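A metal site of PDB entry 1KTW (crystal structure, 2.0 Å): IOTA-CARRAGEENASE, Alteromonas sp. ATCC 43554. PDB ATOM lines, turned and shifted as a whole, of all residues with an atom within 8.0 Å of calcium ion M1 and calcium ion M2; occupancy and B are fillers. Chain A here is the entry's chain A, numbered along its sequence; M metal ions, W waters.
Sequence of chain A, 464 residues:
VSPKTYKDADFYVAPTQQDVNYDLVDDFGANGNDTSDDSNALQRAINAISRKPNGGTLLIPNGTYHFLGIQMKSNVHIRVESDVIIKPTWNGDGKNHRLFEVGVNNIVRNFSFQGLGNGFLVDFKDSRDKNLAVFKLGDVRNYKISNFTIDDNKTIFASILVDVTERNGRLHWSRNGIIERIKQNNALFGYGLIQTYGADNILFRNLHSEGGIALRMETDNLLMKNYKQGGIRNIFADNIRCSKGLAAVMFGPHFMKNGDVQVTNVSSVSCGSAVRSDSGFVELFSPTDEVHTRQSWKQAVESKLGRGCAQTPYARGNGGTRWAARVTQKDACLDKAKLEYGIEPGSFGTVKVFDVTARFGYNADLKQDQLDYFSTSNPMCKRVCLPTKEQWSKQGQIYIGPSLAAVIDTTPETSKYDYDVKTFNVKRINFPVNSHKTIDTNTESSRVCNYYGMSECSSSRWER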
ATOM      1  N   SER A 277      -8.211 -19.383 -15.208  1.00  0.00           N
ATOM      2  CA  SER A 277      -8.941 -20.241 -16.161  1.00  0.00           C
ATOM      3  C   SER A 277     -10.158 -19.487 -16.703  1.00  0.00           C
ATOM      4  O   SER A 277     -10.995 -19.031 -15.933  1.00  0.00           O
ATOM      5  CB  SER A 277      -9.393 -21.555 -15.489  1.00  0.00           C
ATOM      6  OG  SER A 277      -8.289 -22.349 -15.042  1.00  0.00           O
ATOM      7  N   ASP A 409     -11.114 -18.417 -11.499  1.00  0.00           N
ATOM      8  CA  ASP A 409     -11.744 -19.441 -12.341  1.00  0.00           C
ATOM      9  C   ASP A 409     -13.150 -19.011 -12.775  1.00  0.00           C
ATOM     10  O   ASP A 409     -14.086 -19.051 -11.983  1.00  0.00           O
ATOM     11  CB  ASP A 409     -11.850 -20.762 -11.555  1.00  0.00           C
ATOM     12  CG  ASP A 409     -12.469 -21.914 -12.368  1.00  0.00           C
ATOM     13  OD1 ASP A 409     -13.195 -21.689 -13.373  1.00  0.00           O
ATOM     14  OD2 ASP A 409     -12.237 -23.073 -11.979  1.00  0.00           O
ATOM     15  N   THR A 410     -13.290 -18.620 -14.040  1.00  0.00           N
ATOM     16  CA  THR A 410     -14.591 -18.192 -14.524  1.00  0.00           C
ATOM     17  C   THR A 410     -15.261 -19.157 -15.484  1.00  0.00           C
ATOM     18  O   THR A 410     -16.010 -18.734 -16.363  1.00  0.00           O
ATOM     19  CB  THR A 410     -14.518 -16.790 -15.181  1.00  0.00           C
ATOM     20  OG1 THR A 410     -13.510 -16.784 -16.196  1.00  0.00           O
ATOM     21  CG2 THR A 410     -14.194 -15.739 -14.117  1.00  0.00           C
ATOM     22  N   THR A 411     -15.010 -20.453 -15.319  1.00  0.00           N
ATOM     23  CA  THR A 411     -15.640 -21.452 -16.174  1.00  0.00           C
ATOM     24  C   THR A 411     -17.091 -21.527 -15.710  1.00  0.00           C
ATOM     25  O   THR A 411     -17.371 -21.420 -14.510  1.00  0.00           O
ATOM     26  CB  THR A 411     -14.956 -22.831 -16.075  1.00  0.00           C
ATOM     27  OG1 THR A 411     -14.910 -23.251 -14.711  1.00  0.00           O
ATOM     28  CG2 THR A 411     -13.523 -22.753 -16.629  1.00  0.00           C
ATOM     29  N   PRO A 412     -18.048 -21.723 -16.655  1.00  0.00           N
ATOM     30  CA  PRO A 412     -19.487 -21.802 -16.370  1.00  0.00           C
ATOM     31  C   PRO A 412     -19.951 -23.085 -15.668  1.00  0.00           C
ATOM     32  O   PRO A 412     -20.543 -23.970 -16.281  1.00  0.00           O
ATOM     33  CB  PRO A 412     -20.114 -21.614 -17.745  1.00  0.00           C
ATOM     34  CG  PRO A 412     -19.157 -22.352 -18.618  1.00  0.00           C
ATOM     35  CD  PRO A 412     -17.797 -21.917 -18.090  1.00  0.00           C
ATOM     36  N   GLU A 413     -19.698 -23.138 -14.357  1.00  0.00           N
ATOM     37  CA  GLU A 413     -20.021 -24.263 -13.498  1.00  0.00           C
ATOM     38  C   GLU A 413     -21.366 -24.965 -13.724  1.00  0.00           C
ATOM     39  O   GLU A 413     -21.425 -26.178 -13.838  1.00  0.00           O
ATOM     40  CB  GLU A 413     -19.950 -23.817 -12.034  1.00  0.00           C
ATOM     41  CG  GLU A 413     -19.961 -24.958 -11.031  1.00  0.00           C
ATOM     42  CD  GLU A 413     -20.124 -24.483  -9.587  1.00  0.00           C
ATOM     43  OE1 GLU A 413     -19.617 -23.392  -9.241  1.00  0.00           O
ATOM     44  OE2 GLU A 413     -20.763 -25.212  -8.794  1.00  0.00           O
ATOM     45  N   THR A 414     -22.442 -24.185 -13.774  1.00  0.00           N
ATOM     46  CA  THR A 414     -23.780 -24.749 -13.946  1.00  0.00           C
ATOM     47  C   THR A 414     -24.197 -24.953 -15.408  1.00  0.00           C
ATOM     48  O   THR A 414     -25.361 -25.193 -15.689  1.00  0.00           O
ATOM     49  CB  THR A 414     -24.848 -23.877 -13.234  1.00  0.00           C
ATOM     50  N   SER A 415     -23.230 -24.856 -16.320  1.00  0.00           N
ATOM     51  CA  SER A 415     -23.495 -25.007 -17.752  1.00  0.00           C
ATOM     52  C   SER A 415     -23.059 -26.351 -18.339  1.00  0.00           C
ATOM     53  O   SER A 415     -22.173 -27.020 -17.805  1.00  0.00           O
ATOM     54  CB  SER A 415     -22.814 -23.891 -18.531  1.00  0.00           C
ATOM     55  OG  SER A 415     -22.854 -24.150 -19.923  1.00  0.00           O
ATOM     56  N   TYR A 417     -21.541 -26.626 -21.066  1.00  0.00           N
ATOM     57  CA  TYR A 417     -20.274 -26.386 -21.757  1.00  0.00           C
ATOM     58  C   TYR A 417     -19.104 -26.154 -20.800  1.00  0.00           C
ATOM     59  O   TYR A 417     -18.041 -25.679 -21.214  1.00  0.00           O
ATOM     60  CB  TYR A 417     -20.377 -25.165 -22.680  1.00  0.00           C
ATOM     61  CG  TYR A 417     -21.423 -25.272 -23.766  1.00  0.00           C
ATOM     62  CD1 TYR A 417     -22.737 -24.849 -23.551  1.00  0.00           C
ATOM     63  CD2 TYR A 417     -21.096 -25.782 -25.024  1.00  0.00           C
ATOM     64  CE1 TYR A 417     -23.700 -24.937 -24.551  1.00  0.00           C
ATOM     65  CE2 TYR A 417     -22.052 -25.881 -26.029  1.00  0.00           C
ATOM     66  CZ  TYR A 417     -23.357 -25.451 -25.786  1.00  0.00           C
ATOM     67  OH  TYR A 417     -24.299 -25.533 -26.790  1.00  0.00           O
ATOM     68  N   ASP A 418     -19.287 -26.493 -19.527  1.00  0.00           N
ATOM     69  CA  ASP A 418     -18.250 -26.305 -18.516  1.00  0.00           C
ATOM     70  C   ASP A 418     -17.076 -27.285 -18.642  1.00  0.00           C
ATOM     71  O   ASP A 418     -17.213 -28.351 -19.250  1.00  0.00           O
ATOM     72  CB  ASP A 418     -18.873 -26.460 -17.104  1.00  0.00           C
ATOM     73  CG  ASP A 418     -17.915 -26.059 -15.970  1.00  0.00           C
ATOM     74  OD1 ASP A 418     -17.292 -24.997 -16.089  1.00  0.00           O
ATOM     75  OD2 ASP A 418     -17.799 -26.798 -14.954  1.00  0.00           O
ATOM     76  N   TYR A 419     -15.922 -26.897 -18.098  1.00  0.00           N
ATOM     77  CA  TYR A 419     -14.748 -27.773 -18.018  1.00  0.00           C
ATOM     78  C   TYR A 419     -14.091 -27.395 -16.684  1.00  0.00           C
ATOM     79  O   TYR A 419     -14.348 -26.300 -16.163  1.00  0.00           O
ATOM     80  CB  TYR A 419     -13.787 -27.609 -19.223  1.00  0.00           C
ATOM     81  CG  TYR A 419     -12.921 -26.371 -19.256  1.00  0.00           C
ATOM     82  CD1 TYR A 419     -13.356 -25.193 -19.877  1.00  0.00           C
ATOM     83  CD2 TYR A 419     -11.669 -26.362 -18.630  1.00  0.00           C
ATOM     84  CE1 TYR A 419     -12.548 -24.037 -19.887  1.00  0.00           C
ATOM     85  CE2 TYR A 419     -10.860 -25.206 -18.640  1.00  0.00           C
ATOM     86  CZ  TYR A 419     -11.303 -24.051 -19.259  1.00  0.00           C
ATOM     87  OH  TYR A 419     -10.495 -22.921 -19.257  1.00  0.00           O
ATOM     88  N   ASP A 420     -13.295 -28.278 -16.103  1.00  0.00           N
ATOM     89  CA  ASP A 420     -12.699 -27.981 -14.802  1.00  0.00           C
ATOM     90  C   ASP A 420     -11.177 -27.994 -14.687  1.00  0.00           C
ATOM     91  O   ASP A 420     -10.494 -28.753 -15.384  1.00  0.00           O
ATOM     92  CB  ASP A 420     -13.260 -28.940 -13.740  1.00  0.00           C
ATOM     93  CG  ASP A 420     -14.789 -28.862 -13.617  1.00  0.00           C
ATOM     94  OD1 ASP A 420     -15.351 -27.764 -13.784  1.00  0.00           O
ATOM     95  OD2 ASP A 420     -15.416 -29.907 -13.339  1.00  0.00           O
ATOM     96  N   VAL A 421     -10.664 -27.140 -13.807  1.00  0.00           N
ATOM     97  CA  VAL A 421      -9.234 -27.019 -13.507  1.00  0.00           C
ATOM     98  C   VAL A 421      -9.143 -27.168 -11.980  1.00  0.00           C
ATOM     99  O   VAL A 421      -9.535 -26.258 -11.233  1.00  0.00           O
ATOM    100  CB  VAL A 421      -8.688 -25.618 -13.927  1.00  0.00           C
ATOM    101  CG1 VAL A 421      -7.260 -25.432 -13.435  1.00  0.00           C
ATOM    102  CG2 VAL A 421      -8.736 -25.466 -15.447  1.00  0.00           C
ATOM    103  N   LYS A 422      -8.651 -28.320 -11.511  1.00  0.00           N
ATOM    104  CA  LYS A 422      -8.555 -28.594 -10.078  1.00  0.00           C
ATOM    105  C   LYS A 422      -7.214 -28.156  -9.494  1.00  0.00           C
ATOM    106  O   LYS A 422      -6.170 -28.462 -10.075  1.00  0.00           O
ATOM    107  CB  LYS A 422      -8.724 -30.096  -9.836  1.00  0.00           C
ATOM    108  CG  LYS A 422      -9.954 -30.687 -10.485  1.00  0.00           C
ATOM    109  CD  LYS A 422     -10.115 -32.155 -10.115  1.00  0.00           C
ATOM    110  CE  LYS A 422     -11.314 -32.784 -10.825  1.00  0.00           C
ATOM    111  NZ  LYS A 422     -11.185 -32.716 -12.305  1.00  0.00           N
ATOM    112  N   THR A 441     -17.258 -17.928 -10.478  1.00  0.00           N
ATOM    113  CA  THR A 441     -18.452 -17.248 -10.962  1.00  0.00           C
ATOM    114  C   THR A 441     -19.498 -16.912  -9.914  1.00  0.00           C
ATOM    115  O   THR A 441     -20.426 -16.163 -10.228  1.00  0.00           O
ATOM    116  CB  THR A 441     -19.155 -18.029 -12.124  1.00  0.00           C
ATOM    117  OG1 THR A 441     -19.610 -19.295 -11.656  1.00  0.00           O
ATOM    118  CG2 THR A 441     -18.196 -18.216 -13.286  1.00  0.00           C
HETATM  119 CA    CA M   1     -15.615 -25.551 -14.063  1.00  0.00          CA
HETATM  120 CA    CA M   2     -17.611 -28.885 -13.657  1.00  0.00          CA
HETATM  121  O   HOH W   1     -20.119 -28.247 -13.232  1.00  0.00           O
HETATM  122  O   HOH W   2     -13.580 -25.311 -12.721  1.00  0.00           O
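The side-chain carboxylate (OD2) of Asp 420 is bound to calcium ion M2, at 2.4 Å.
Calcium ion M2 is bound by OD2 of Asp 418 (2.5 Å).
OD1 of Asp 420 binds calcium ion M2.
Calcium ion M2 is bound by water W1 (2.6 Å).
Two residues have an atom within 4 Å of calcium ion M2: Asp 418 and Asp 420.
The nearest printed residue that does not touch calcium ion M2 is Glu 413 (4.7 Å).
Calcium ion M1 is bound by the side-chain carboxylate (OD1) of Asp 420 (2.2 Å), water W2 (2.4 Å), the side-chain hydroxyl (OG1) of Thr 411 (2.5 Å), the backbone carbonyl oxygen (O) of Tyr 419 (2.6 Å), the side-chain carboxylate (OD2) of Asp 418 (2.7 Å) and the side-chain carboxylate (OD1) of Asp 418 (2.7 Å).
OD1 of Asp 409 lies within hydrogen-bond range of N of Thr 411 (2.9 Å).
The side-chain carboxylate of Asp 418 sits close to the backbone NH of Glu 413 (3.5 Å).
Of the 15 residues printed, 4 come within 4 Å of calcium ion M1.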
